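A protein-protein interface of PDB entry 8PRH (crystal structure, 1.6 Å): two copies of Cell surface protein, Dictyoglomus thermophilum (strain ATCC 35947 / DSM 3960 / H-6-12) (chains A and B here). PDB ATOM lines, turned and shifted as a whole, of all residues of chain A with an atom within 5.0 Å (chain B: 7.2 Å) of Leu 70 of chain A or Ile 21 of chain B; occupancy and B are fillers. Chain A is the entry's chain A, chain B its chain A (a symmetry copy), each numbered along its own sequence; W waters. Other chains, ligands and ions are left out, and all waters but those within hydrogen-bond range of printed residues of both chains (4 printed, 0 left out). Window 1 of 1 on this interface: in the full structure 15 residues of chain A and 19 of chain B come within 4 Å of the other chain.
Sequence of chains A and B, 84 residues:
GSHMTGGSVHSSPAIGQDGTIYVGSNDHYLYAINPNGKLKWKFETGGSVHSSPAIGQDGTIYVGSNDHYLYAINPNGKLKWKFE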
ATOM      1  N   TYR A  62      -0.850 -31.024 -22.735  1.00  0.00           N
ATOM      2  CA  TYR A  62      -1.713 -29.858 -22.846  1.00  0.00           C
ATOM      3  C   TYR A  62      -1.521 -29.215 -24.207  1.00  0.00           C
ATOM      4  O   TYR A  62      -0.383 -29.009 -24.648  1.00  0.00           O
ATOM      5  CB  TYR A  62      -1.394 -28.818 -21.771  1.00  0.00           C
ATOM      6  CG  TYR A  62      -1.391 -29.345 -20.378  1.00  0.00           C
ATOM      7  CD1 TYR A  62      -2.583 -29.445 -19.667  1.00  0.00           C
ATOM      8  CD2 TYR A  62      -0.205 -29.797 -19.787  1.00  0.00           C
ATOM      9  CE1 TYR A  62      -2.589 -29.930 -18.368  1.00  0.00           C
ATOM     10  CE2 TYR A  62      -0.188 -30.285 -18.478  1.00  0.00           C
ATOM     11  CZ  TYR A  62      -1.393 -30.370 -17.803  1.00  0.00           C
ATOM     12  OH  TYR A  62      -1.397 -30.836 -16.517  1.00  0.00           O
ATOM     13  N   VAL A  63      -2.626 -28.890 -24.878  1.00  0.00           N
ATOM     14  CA  VAL A  63      -2.509 -28.171 -26.143  1.00  0.00           C
ATOM     15  C   VAL A  63      -3.784 -27.382 -26.392  1.00  0.00           C
ATOM     16  O   VAL A  63      -4.885 -27.812 -26.028  1.00  0.00           O
ATOM     17  CB  VAL A  63      -2.191 -29.159 -27.294  1.00  0.00           C
ATOM     18  CG1 VAL A  63      -3.419 -29.969 -27.689  1.00  0.00           C
ATOM     19  CG2 VAL A  63      -1.557 -28.421 -28.484  1.00  0.00           C
ATOM     20  N   GLY A  64      -3.623 -26.215 -27.016  1.00  0.00           N
ATOM     21  CA  GLY A  64      -4.776 -25.419 -27.403  1.00  0.00           C
ATOM     22  C   GLY A  64      -5.243 -25.788 -28.797  1.00  0.00           C
ATOM     23  O   GLY A  64      -4.471 -26.282 -29.621  1.00  0.00           O
ATOM     24  N   HIS A  68     -11.197 -23.156 -29.517  1.00  0.00           N
ATOM     25  CA  HIS A  68     -11.108 -22.197 -28.415  1.00  0.00           C
ATOM     26  C   HIS A  68     -10.909 -22.875 -27.064  1.00  0.00           C
ATOM     27  O   HIS A  68     -10.936 -22.204 -26.030  1.00  0.00           O
ATOM     28  CB  HIS A  68     -12.334 -21.272 -28.348  1.00  0.00           C
ATOM     29  CG  HIS A  68     -12.371 -20.257 -29.446  1.00  0.00           C
ATOM     30  ND1 HIS A  68     -12.974 -19.026 -29.307  1.00  0.00           N
ATOM     31  CD2 HIS A  68     -11.917 -20.311 -30.721  1.00  0.00           C
ATOM     32  CE1 HIS A  68     -12.864 -18.353 -30.439  1.00  0.00           C
ATOM     33  NE2 HIS A  68     -12.232 -19.112 -31.316  1.00  0.00           N
ATOM     34  N   TYR A  69     -10.657 -24.182 -27.049  1.00  0.00           N
ATOM     35  CA  TYR A  69     -10.431 -24.901 -25.797  1.00  0.00           C
ATOM     36  C   TYR A  69      -8.944 -25.156 -25.608  1.00  0.00           C
ATOM     37  O   TYR A  69      -8.234 -25.432 -26.581  1.00  0.00           O
ATOM     38  CB  TYR A  69     -11.153 -26.244 -25.825  1.00  0.00           C
ATOM     39  CG  TYR A  69     -12.628 -26.180 -25.497  1.00  0.00           C
ATOM     40  CD1 TYR A  69     -13.080 -25.866 -24.226  1.00  0.00           C
ATOM     41  CD2 TYR A  69     -13.560 -26.290 -26.521  1.00  0.00           C
ATOM     42  CE1 TYR A  69     -14.438 -25.795 -23.958  1.00  0.00           C
ATOM     43  CE2 TYR A  69     -14.920 -26.194 -26.269  1.00  0.00           C
ATOM     44  CZ  TYR A  69     -15.345 -25.941 -24.996  1.00  0.00           C
ATOM     45  OH  TYR A  69     -16.701 -25.851 -24.769  1.00  0.00           O
ATOM     46  N   LEU A  70      -8.492 -25.066 -24.353  1.00  0.00           N
ATOM     47  CA  LEU A  70      -7.217 -25.648 -23.935  1.00  0.00           C
ATOM     48  C   LEU A  70      -7.497 -27.053 -23.419  1.00  0.00           C
ATOM     49  O   LEU A  70      -8.271 -27.228 -22.468  1.00  0.00           O
ATOM     50  CB  LEU A  70      -6.525 -24.805 -22.864  1.00  0.00           C
ATOM     51  CG  LEU A  70      -5.242 -25.507 -22.425  1.00  0.00           C
ATOM     52  CD1 LEU A  70      -4.123 -25.188 -23.420  1.00  0.00           C
ATOM     53  CD2 LEU A  70      -4.838 -25.130 -21.035  1.00  0.00           C
ATOM     54  N   TYR A  71      -6.895 -28.049 -24.062  1.00  0.00           N
ATOM     55  CA  TYR A  71      -7.107 -29.458 -23.720  1.00  0.00           C
ATOM     56  C   TYR A  71      -6.023 -29.988 -22.790  1.00  0.00           C
ATOM     57  O   TYR A  71      -4.832 -29.709 -22.974  1.00  0.00           O
ATOM     58  CB  TYR A  71      -7.109 -30.322 -24.993  1.00  0.00           C
ATOM     59  CG  TYR A  71      -8.367 -30.172 -25.820  1.00  0.00           C
ATOM     60  CD1 TYR A  71      -8.468 -29.170 -26.777  1.00  0.00           C
ATOM     61  CD2 TYR A  71      -9.454 -30.998 -25.601  1.00  0.00           C
ATOM     62  CE1 TYR A  71      -9.619 -29.017 -27.515  1.00  0.00           C
ATOM     63  CE2 TYR A  71     -10.603 -30.854 -26.333  1.00  0.00           C
ATOM     64  CZ  TYR A  71     -10.675 -29.864 -27.280  1.00  0.00           C
ATOM     65  OH  TYR A  71     -11.846 -29.740 -27.998  1.00  0.00           O
ATOM     66  N   ALA A  72      -6.451 -30.782 -21.805  1.00  0.00           N
ATOM     67  CA  ALA A  72      -5.552 -31.628 -21.017  1.00  0.00           C
ATOM     68  C   ALA A  72      -5.899 -33.063 -21.352  1.00  0.00           C
ATOM     69  O   ALA A  72      -7.033 -33.488 -21.135  1.00  0.00           O
ATOM     70  CB  ALA A  72      -5.741 -31.365 -19.524  1.00  0.00           C
ATOM     71  N   TRP A  81      -9.500 -32.950 -19.186  1.00  0.00           N
ATOM     72  CA  TRP A  81     -10.463 -31.854 -19.110  1.00  0.00           C
ATOM     73  C   TRP A  81     -10.199 -30.892 -20.254  1.00  0.00           C
ATOM     74  O   TRP A  81      -9.167 -30.969 -20.939  1.00  0.00           O
ATOM     75  CB  TRP A  81     -10.415 -31.126 -17.742  1.00  0.00           C
ATOM     76  CG  TRP A  81      -9.050 -30.743 -17.215  1.00  0.00           C
ATOM     77  CD1 TRP A  81      -8.418 -31.326 -16.176  1.00  0.00           C
ATOM     78  CD2 TRP A  81      -8.164 -29.675 -17.679  1.00  0.00           C
ATOM     79  NE1 TRP A  81      -7.202 -30.714 -15.940  1.00  0.00           N
ATOM     80  CE2 TRP A  81      -7.030 -29.690 -16.830  1.00  0.00           C
ATOM     81  CE3 TRP A  81      -8.246 -28.696 -18.682  1.00  0.00           C
ATOM     82  CZ2 TRP A  81      -5.948 -28.801 -16.984  1.00  0.00           C
ATOM     83  CZ3 TRP A  81      -7.146 -27.794 -18.849  1.00  0.00           C
ATOM     84  CH2 TRP A  81      -6.031 -27.853 -17.984  1.00  0.00           C
ATOM     85  N   LYS A  82     -11.160 -29.990 -20.488  1.00  0.00           N
ATOM     86  CA  LYS A  82     -10.921 -28.908 -21.424  1.00  0.00           C
ATOM     87  C   LYS A  82     -11.299 -27.604 -20.742  1.00  0.00           C
ATOM     88  O   LYS A  82     -12.178 -27.565 -19.875  1.00  0.00           O
ATOM     89  CB  LYS A  82     -11.678 -29.087 -22.749  1.00  0.00           C
ATOM     90  CG  LYS A  82     -13.162 -29.320 -22.633  1.00  0.00           C
ATOM     91  CD  LYS A  82     -13.675 -29.934 -23.928  1.00  0.00           C
ATOM     92  CE  LYS A  82     -15.182 -29.957 -23.959  1.00  0.00           C
ATOM     93  NZ  LYS A  82     -15.654 -30.708 -25.156  1.00  0.00           N
ATOM     94  N   PHE A  83     -10.566 -26.556 -21.080  1.00  0.00           N
ATOM     95  CA  PHE A  83     -10.738 -25.263 -20.441  1.00  0.00           C
ATOM     96  C   PHE A  83     -11.112 -24.230 -21.492  1.00  0.00           C
ATOM     97  O   PHE A  83     -10.440 -24.113 -22.515  1.00  0.00           O
ATOM     98  CB  PHE A  83      -9.447 -24.849 -19.703  1.00  0.00           C
ATOM     99  CG  PHE A  83      -9.541 -23.485 -19.100  1.00  0.00           C
ATOM    100  CD1 PHE A  83     -10.032 -23.321 -17.813  1.00  0.00           C
ATOM    101  CD2 PHE A  83      -9.176 -22.367 -19.836  1.00  0.00           C
ATOM    102  CE1 PHE A  83     -10.169 -22.037 -17.271  1.00  0.00           C
ATOM    103  CE2 PHE A  83      -9.289 -21.095 -19.293  1.00  0.00           C
ATOM    104  CZ  PHE A  83      -9.791 -20.932 -18.022  1.00  0.00           C
ATOM    105  N   HIS B  10      -4.581 -20.002 -29.470  1.00  0.00           N
ATOM    106  CA  HIS B  10      -3.698 -20.217 -28.333  1.00  0.00           C
ATOM    107  C   HIS B  10      -2.232 -20.186 -28.737  1.00  0.00           C
ATOM    108  O   HIS B  10      -1.846 -20.645 -29.819  1.00  0.00           O
ATOM    109  CB  HIS B  10      -3.957 -21.561 -27.652  1.00  0.00           C
ATOM    110  CG  HIS B  10      -5.356 -21.740 -27.150  1.00  0.00           C
ATOM    111  ND1 HIS B  10      -6.348 -22.338 -27.906  1.00  0.00           N
ATOM    112  CD2 HIS B  10      -5.918 -21.451 -25.951  1.00  0.00           C
ATOM    113  CE1 HIS B  10      -7.460 -22.401 -27.198  1.00  0.00           C
ATOM    114  NE2 HIS B  10      -7.227 -21.875 -26.004  1.00  0.00           N
ATOM    115  N   SER B  11      -1.421 -19.658 -27.832  1.00  0.00           N
ATOM    116  CA  SER B  11       0.010 -19.877 -27.844  1.00  0.00           C
ATOM    117  C   SER B  11       0.286 -21.314 -27.409  1.00  0.00           C
ATOM    118  O   SER B  11      -0.620 -22.070 -27.043  1.00  0.00           O
ATOM    119  CB  SER B  11       0.681 -18.863 -26.911  1.00  0.00           C
ATOM    120  OG  SER B  11       0.643 -19.285 -25.546  1.00  0.00           O
ATOM    121  N   SER B  12       1.516 -21.686 -27.477  1.00  0.00           N
ATOM    122  CA  SER B  12       1.866 -22.959 -26.884  1.00  0.00           C
ATOM    123  C   SER B  12       1.930 -22.798 -25.371  1.00  0.00           C
ATOM    124  O   SER B  12       2.335 -21.739 -24.886  1.00  0.00           O
ATOM    125  CB  SER B  12       3.195 -23.430 -27.436  1.00  0.00           C
ATOM    126  OG  SER B  12       3.127 -23.316 -28.849  1.00  0.00           O
ATOM    127  N   PRO B  13       1.512 -23.791 -24.596  1.00  0.00           N
ATOM    128  CA  PRO B  13       1.529 -23.628 -23.143  1.00  0.00           C
ATOM    129  C   PRO B  13       2.920 -23.817 -22.575  1.00  0.00           C
ATOM    130  O   PRO B  13       3.799 -24.462 -23.169  1.00  0.00           O
ATOM    131  CB  PRO B  13       0.581 -24.722 -22.613  1.00  0.00           C
ATOM    132  CG  PRO B  13       0.078 -25.474 -23.836  1.00  0.00           C
ATOM    133  CD  PRO B  13       0.795 -25.004 -25.041  1.00  0.00           C
ATOM    134  N   ALA B  14       3.098 -23.257 -21.379  1.00  0.00           N
ATOM    135  CA  ALA B  14       4.284 -23.470 -20.560  1.00  0.00           C
ATOM    136  C   ALA B  14       3.847 -24.027 -19.219  1.00  0.00           C
ATOM    137  O   ALA B  14       2.754 -23.699 -18.752  1.00  0.00           O
ATOM    138  CB  ALA B  14       5.086 -22.150 -20.345  1.00  0.00           C
ATOM    139  N   ILE B  15       4.701 -24.839 -18.587  1.00  0.00           N
ATOM    140  CA  ILE B  15       4.356 -25.521 -17.345  1.00  0.00           C
ATOM    141  C   ILE B  15       5.239 -25.001 -16.219  1.00  0.00           C
ATOM    142  O   ILE B  15       6.477 -25.038 -16.330  1.00  0.00           O
ATOM    143  CB  ILE B  15       4.523 -27.045 -17.478  1.00  0.00           C
ATOM    144  CG1 ILE B  15       3.815 -27.574 -18.742  1.00  0.00           C
ATOM    145  CG2 ILE B  15       4.003 -27.709 -16.229  1.00  0.00           C
ATOM    146  CD1 ILE B  15       2.312 -27.264 -18.794  1.00  0.00           C
ATOM    147  N   GLY B  16       4.605 -24.572 -15.108  1.00  0.00           N
ATOM    148  CA  GLY B  16       5.339 -24.092 -13.947  1.00  0.00           C
ATOM    149  C   GLY B  16       5.764 -25.222 -13.013  1.00  0.00           C
ATOM    150  O   GLY B  16       5.442 -26.394 -13.222  1.00  0.00           O
ATOM    151  N   ASP B  18       4.819 -26.170 -10.104  1.00  0.00           N
ATOM    152  CA  ASP B  18       3.750 -26.884  -9.425  1.00  0.00           C
ATOM    153  C   ASP B  18       2.761 -27.462 -10.407  1.00  0.00           C
ATOM    154  O   ASP B  18       1.680 -27.891  -9.999  1.00  0.00           O
ATOM    155  CB  ASP B  18       3.018 -25.982  -8.410  1.00  0.00           C
ATOM    156  CG  ASP B  18       2.349 -24.759  -9.050  1.00  0.00           C
ATOM    157  OD1 ASP B  18       2.538 -24.532 -10.268  1.00  0.00           O
ATOM    158  OD2 ASP B  18       1.659 -24.017  -8.329  1.00  0.00           O
ATOM    159  N   GLY B  19       3.109 -27.460 -11.688  1.00  0.00           N
ATOM    160  CA  GLY B  19       2.231 -27.975 -12.709  1.00  0.00           C
ATOM    161  C   GLY B  19       1.296 -26.952 -13.332  1.00  0.00           C
ATOM    162  O   GLY B  19       0.540 -27.317 -14.228  1.00  0.00           O
ATOM    163  N   THR B  20       1.306 -25.693 -12.875  1.00  0.00           N
ATOM    164  CA  THR B  20       0.420 -24.686 -13.452  1.00  0.00           C
ATOM    165  C   THR B  20       0.675 -24.579 -14.943  1.00  0.00           C
ATOM    166  O   THR B  20       1.827 -24.607 -15.385  1.00  0.00           O
ATOM    167  CB  THR B  20       0.649 -23.317 -12.778  1.00  0.00           C
ATOM    168  OG1 THR B  20       0.387 -23.434 -11.373  1.00  0.00           O
ATOM    169  CG2 THR B  20      -0.283 -22.229 -13.351  1.00  0.00           C
ATOM    170  N   ILE B  21      -0.404 -24.427 -15.712  1.00  0.00           N
ATOM    171  CA  ILE B  21      -0.331 -24.342 -17.162  1.00  0.00           C
ATOM    172  C   ILE B  21      -0.588 -22.895 -17.547  1.00  0.00           C
ATOM    173  O   ILE B  21      -1.647 -22.331 -17.243  1.00  0.00           O
ATOM    174  CB  ILE B  21      -1.349 -25.286 -17.825  1.00  0.00           C
ATOM    175  CG1 ILE B  21      -1.167 -26.732 -17.342  1.00  0.00           C
ATOM    176  CG2 ILE B  21      -1.220 -25.200 -19.348  1.00  0.00           C
ATOM    177  CD1 ILE B  21      -2.168 -27.128 -16.218  1.00  0.00           C
ATOM    178  N   TYR B  22       0.384 -22.276 -18.216  1.00  0.00           N
ATOM    179  CA  TYR B  22       0.255 -20.904 -18.674  1.00  0.00           C
ATOM    180  C   TYR B  22       0.094 -20.868 -20.179  1.00  0.00           C
ATOM    181  O   TYR B  22       0.881 -21.505 -20.898  1.00  0.00           O
ATOM    182  CB  TYR B  22       1.496 -20.099 -18.312  1.00  0.00           C
ATOM    183  CG  TYR B  22       1.852 -20.133 -16.855  1.00  0.00           C
ATOM    184  CD1 TYR B  22       1.234 -19.281 -15.933  1.00  0.00           C
ATOM    185  CD2 TYR B  22       2.844 -21.015 -16.397  1.00  0.00           C
ATOM    186  CE1 TYR B  22       1.601 -19.335 -14.581  1.00  0.00           C
ATOM    187  CE2 TYR B  22       3.229 -21.042 -15.050  1.00  0.00           C
ATOM    188  CZ  TYR B  22       2.598 -20.221 -14.148  1.00  0.00           C
ATOM    189  OH  TYR B  22       3.000 -20.241 -12.815  1.00  0.00           O
ATOM    190  N   VAL B  23      -0.921 -20.151 -20.658  1.00  0.00           N
ATOM    191  CA  VAL B  23      -1.143 -20.097 -22.103  1.00  0.00           C
ATOM    192  C   VAL B  23      -1.698 -18.733 -22.472  1.00  0.00           C
ATOM    193  O   VAL B  23      -2.551 -18.183 -21.763  1.00  0.00           O
ATOM    194  CB  VAL B  23      -2.064 -21.242 -22.564  1.00  0.00           C
ATOM    195  CG1 VAL B  23      -3.487 -21.064 -21.986  1.00  0.00           C
ATOM    196  CG2 VAL B  23      -2.034 -21.342 -24.113  1.00  0.00           C
ATOM    197  N   LEU B  30      -3.359 -13.606 -20.758  1.00  0.00           N
ATOM    198  CA  LEU B  30      -2.528 -14.745 -20.384  1.00  0.00           C
ATOM    199  C   LEU B  30      -3.255 -15.500 -19.282  1.00  0.00           C
ATOM    200  O   LEU B  30      -3.650 -14.890 -18.283  1.00  0.00           O
ATOM    201  CB  LEU B  30      -1.159 -14.265 -19.881  1.00  0.00           C
ATOM    202  CG  LEU B  30      -0.318 -15.376 -19.251  1.00  0.00           C
ATOM    203  CD1 LEU B  30       0.164 -16.291 -20.379  1.00  0.00           C
ATOM    204  CD2 LEU B  30       0.847 -14.771 -18.465  1.00  0.00           C
ATOM    205  N   TYR B  31      -3.466 -16.806 -19.477  1.00  0.00           N
ATOM    206  CA  TYR B  31      -4.192 -17.640 -18.519  1.00  0.00           C
ATOM    207  C   TYR B  31      -3.222 -18.486 -17.714  1.00  0.00           C
ATOM    208  O   TYR B  31      -2.263 -19.020 -18.265  1.00  0.00           O
ATOM    209  CB  TYR B  31      -5.184 -18.553 -19.250  1.00  0.00           C
ATOM    210  CG  TYR B  31      -6.343 -17.808 -19.837  1.00  0.00           C
ATOM    211  CD1 TYR B  31      -7.501 -17.605 -19.093  1.00  0.00           C
ATOM    212  CD2 TYR B  31      -6.275 -17.306 -21.135  1.00  0.00           C
ATOM    213  CE1 TYR B  31      -8.566 -16.920 -19.631  1.00  0.00           C
ATOM    214  CE2 TYR B  31      -7.349 -16.603 -21.690  1.00  0.00           C
ATOM    215  CZ  TYR B  31      -8.479 -16.435 -20.930  1.00  0.00           C
ATOM    216  OH  TYR B  31      -9.529 -15.730 -21.473  1.00  0.00           O
ATOM    217  N   ALA B  32      -3.474 -18.592 -16.406  1.00  0.00           N
ATOM    218  CA  ALA B  32      -2.775 -19.543 -15.545  1.00  0.00           C
ATOM    219  C   ALA B  32      -3.822 -20.526 -15.045  1.00  0.00           C
ATOM    220  O   ALA B  32      -4.760 -20.128 -14.357  1.00  0.00           O
ATOM    221  CB  ALA B  32      -2.071 -18.825 -14.394  1.00  0.00           C
ATOM    222  N   ILE B  33      -3.666 -21.789 -15.416  1.00  0.00           N
ATOM    223  CA  ILE B  33      -4.667 -22.825 -15.137  1.00  0.00           C
ATOM    224  C   ILE B  33      -4.056 -23.847 -14.177  1.00  0.00           C
ATOM    225  O   ILE B  33      -2.931 -24.310 -14.384  1.00  0.00           O
ATOM    226  CB  ILE B  33      -5.134 -23.485 -16.441  1.00  0.00           C
ATOM    227  CG1 ILE B  33      -5.563 -22.414 -17.446  1.00  0.00           C
ATOM    228  CG2 ILE B  33      -6.271 -24.496 -16.160  1.00  0.00           C
ATOM    229  CD1 ILE B  33      -5.731 -22.931 -18.864  1.00  0.00           C
ATOM    230  N   ASN B  34      -4.795 -24.171 -13.106  1.00  0.00           N
ATOM    231  CA  ASN B  34      -4.431 -25.249 -12.188  1.00  0.00           C
ATOM    232  C   ASN B  34      -4.421 -26.580 -12.939  1.00  0.00           C
ATOM    233  O   ASN B  34      -5.186 -26.764 -13.882  1.00  0.00           O
ATOM    234  CB  ASN B  34      -5.460 -25.285 -11.049  1.00  0.00           C
ATOM    235  CG  ASN B  34      -5.058 -26.187  -9.856  1.00  0.00           C
ATOM    236  OD1 ASN B  34      -4.831 -27.404  -9.978  1.00  0.00           O
ATOM    237  ND2 ASN B  34      -5.067 -25.590  -8.670  1.00  0.00           N
ATOM    238  N   PRO B  35      -3.547 -27.521 -12.562  1.00  0.00           N
ATOM    239  CA  PRO B  35      -3.593 -28.845 -13.206  1.00  0.00           C
ATOM    240  C   PRO B  35      -4.952 -29.530 -13.080  1.00  0.00           C
ATOM    241  O   PRO B  35      -5.250 -30.428 -13.877  1.00  0.00           O
ATOM    242  CB  PRO B  35      -2.489 -29.639 -12.485  1.00  0.00           C
ATOM    243  CG  PRO B  35      -1.650 -28.632 -11.774  1.00  0.00           C
ATOM    244  CD  PRO B  35      -2.436 -27.371 -11.609  1.00  0.00           C
ATOM    245  N   ASN B  36      -5.800 -29.115 -12.122  1.00  0.00           N
ATOM    246  CA  ASN B  36      -7.147 -29.674 -12.037  1.00  0.00           C
ATOM    247  C   ASN B  36      -8.134 -29.064 -13.029  1.00  0.00           C
ATOM    248  O   ASN B  36      -9.310 -29.467 -13.031  1.00  0.00           O
ATOM    249  CB  ASN B  36      -7.675 -29.545 -10.579  1.00  0.00           C
ATOM    250  CG  ASN B  36      -7.896 -28.100 -10.140  1.00  0.00           C
ATOM    251  OD1 ASN B  36      -7.911 -27.171 -10.952  1.00  0.00           O
ATOM    252  ND2 ASN B  36      -8.096 -27.906  -8.828  1.00  0.00           N
ATOM    253  N   GLY B  37      -7.710 -28.112 -13.877  1.00  0.00           N
ATOM    254  CA  GLY B  37      -8.574 -27.548 -14.898  1.00  0.00           C
ATOM    255  C   GLY B  37      -9.335 -26.305 -14.497  1.00  0.00           C
ATOM    256  O   GLY B  37     -10.100 -25.780 -15.321  1.00  0.00           O
ATOM    257  N   LYS B  40      -6.547 -20.354 -12.246  1.00  0.00           N
ATOM    258  CA  LYS B  40      -5.825 -19.746 -11.136  1.00  0.00           C
ATOM    259  C   LYS B  40      -5.928 -18.231 -11.210  1.00  0.00           C
ATOM    260  O   LYS B  40      -6.332 -17.580 -10.239  1.00  0.00           O
ATOM    261  CB  LYS B  40      -4.354 -20.165 -11.137  1.00  0.00           C
ATOM    262  CG  LYS B  40      -3.611 -19.740  -9.872  1.00  0.00           C
ATOM    263  CD  LYS B  40      -2.135 -20.163  -9.833  1.00  0.00           C
ATOM    264  CE  LYS B  40      -2.011 -21.617 -10.081  1.00  0.00           C
ATOM    265  NZ  LYS B  40      -1.538 -22.385  -8.894  1.00  0.00           N
ATOM    266  N   TRP B  41      -5.581 -17.671 -12.365  1.00  0.00           N
ATOM    267  CA  TRP B  41      -5.803 -16.256 -12.631  1.00  0.00           C
ATOM    268  C   TRP B  41      -5.682 -16.021 -14.121  1.00  0.00           C
ATOM    269  O   TRP B  41      -5.188 -16.864 -14.865  1.00  0.00           O
ATOM    270  CB  TRP B  41      -4.795 -15.357 -11.892  1.00  0.00           C
ATOM    271  CG  TRP B  41      -3.341 -15.776 -11.947  1.00  0.00           C
ATOM    272  CD1 TRP B  41      -2.642 -16.366 -10.951  1.00  0.00           C
ATOM    273  CD2 TRP B  41      -2.406 -15.571 -13.031  1.00  0.00           C
ATOM    274  NE1 TRP B  41      -1.329 -16.578 -11.331  1.00  0.00           N
ATOM    275  CE2 TRP B  41      -1.154 -16.075 -12.594  1.00  0.00           C
ATOM    276  CE3 TRP B  41      -2.500 -14.991 -14.308  1.00  0.00           C
ATOM    277  CZ2 TRP B  41       0.000 -16.053 -13.399  1.00  0.00           C
ATOM    278  CZ3 TRP B  41      -1.341 -14.961 -15.118  1.00  0.00           C
ATOM    279  CH2 TRP B  41      -0.106 -15.494 -14.648  1.00  0.00           C
ATOM    280  N   PRO B  53       4.551 -18.441 -23.500  1.00  0.00           N
ATOM    281  CA  PRO B  53       5.246 -17.935 -22.303  1.00  0.00           C
ATOM    282  C   PRO B  53       6.505 -18.720 -21.993  1.00  0.00           C
ATOM    283  O   PRO B  53       6.631 -19.908 -22.303  1.00  0.00           O
ATOM    284  CB  PRO B  53       4.214 -18.075 -21.177  1.00  0.00           C
ATOM    285  CG  PRO B  53       3.048 -18.813 -21.766  1.00  0.00           C
ATOM    286  CD  PRO B  53       3.190 -18.920 -23.240  1.00  0.00           C
HETATM  287  O   HOH W   1       0.832 -29.991 -15.159  1.00  0.00           O
HETATM  288  O   HOH W   2      -3.466 -31.902 -15.464  1.00  0.00           O
HETATM  289  O   HOH W   3      -8.882 -21.616 -23.746  1.00  0.00           O
HETATM  290  O   HOH W   4     -11.594 -27.494 -16.903  1.00  0.00           O
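Among the printed residues, pairs that only touch across the chains: Tyr 69 of chain A with His 10 of chain B (3.2 Å), Leu 70 of chain A with Ile 33 of chain B (3.2 Å), Trp 81 of chain A with Asn 36 of chain B (3.5 Å), His 68 of chain A with His 10 of chain B (3.5 Å), Gly 64 of chain A with His 10 of chain B (3.5 Å), Phe 83 of chain A with Gly 37 of chain B (3.5 Å), Tyr 62 of chain A with Ile 21 of chain B (3.6 Å), Phe 83 of chain A with Ile 33 of chain B (3.6 Å), Tyr 62 of chain A with Pro 13 of chain B (3.7 Å), Tyr 62 of chain A with Ile 15 of chain B (3.7 Å), Trp 81 of chain A with Asn 34 of chain B (3.8 Å), Leu 70 of chain A with His 10 of chain B (3.8 Å), Trp 81 of chain A with Ile 33 of chain B (3.8 Å), Phe 83 of chain A with Tyr 31 of chain B (3.9 Å) and Leu 70 of chain A with Ile 21 of chain B (3.99 Å).
Of the 11 printed residues of chain A, 7 touch a printed residue of chain B.
Hydrophobic or aromatic side chains of chain A that line the printed part of chain B: Tyr 62, Leu 70, Trp 81 and Phe 83.
Hydrophobic or aromatic side chains of chain B that line the printed part of chain A: His 10, Pro 13, Ile 15, Ile 21, Tyr 31 and Ile 33.
Along chain B the printed residues that touch a printed residue of chain A span positions 10 to 37.
Among the printed residues, 17 pairs touch across the chains.
Among the printed residues, no Asp or Glu carboxylate lies within 4 Å of a Lys or Arg side-chain nitrogen of the other chain.
Of the printed residues of chain B, Gly 64 of chain A touches His 10.
Printed residues of chain B within 4 Å of Leu 70 of chain A: His 10 (3.8 Å), Ile 21 (3.99 Å) and Ile 33 (3.2 Å).
Lys 82 of chain A touches none of the printed residues of chain B.
Of the printed residues of chain A, Pro 13 of chain B touches Tyr 62 (3.7 Å).
Of the printed residues of chain A, Ile 21 of chain B touches Tyr 62 and Leu 70.
The nearest printed residue of chain A that does not touch Ile 21 of chain B is Trp 81 of chain A (4.2 Å).
Water W2 lies within hydrogen-bond range of the side-chain hydroxyl of Tyr 62 of chain A (2.6 Å) and the backbone carbonyl oxygen of Pro 35 of chain B (2.8 Å).
Water W1 bridges the side-chain hydroxyl (OH) of Tyr 62 of chain A (2.7 Å) and the backbone carbonyl oxygen (O) of Gly 19 of chain B (2.8 Å).
Water W4 lies within hydrogen-bond range of O of Gly 37 of chain B and O of Lys 82 of chain A.
Water W3 lies within hydrogen-bond range of NE2 of His 10 of chain B, O of His 68 of chain A and O of Phe 83 of chain A.
N of Phe 83 of chain A lies within hydrogen-bond range of O of Leu 70 of chain A, at 2.8 Å.
The backbone NH (N) of Ala 72 of chain A lies within hydrogen-bond range of the backbone carbonyl oxygen (O) of Trp 81 of chain A (2.9 Å).
O of Ile 21 of chain B sits at hydrogen-bond distance from N of Ile 33 of chain B, at 2.8 Å.
O of Val 23 of chain B sits at hydrogen-bond distance from N of Tyr 31 of chain B (2.8 Å).
The side-chain amide oxygen (OD1) of Asn 34 of chain B is in hydrogen-bond range of the backbone NH (N) of Asn 36 of chain B (2.9 Å).
The indole nitrogen (NE1) of Trp 81 of chain A lies within hydrogen-bond range of the backbone carbonyl oxygen (O) of Pro 35 of chain B.
NE1 of Trp 81 of chain A lies close to N of Gly 37 of chain B (3.4 Å).
No position is printed for both chains.
Of the 17 pairs that touch across the chains among the printed residues, none has its exchanged pair printed and touching as well.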
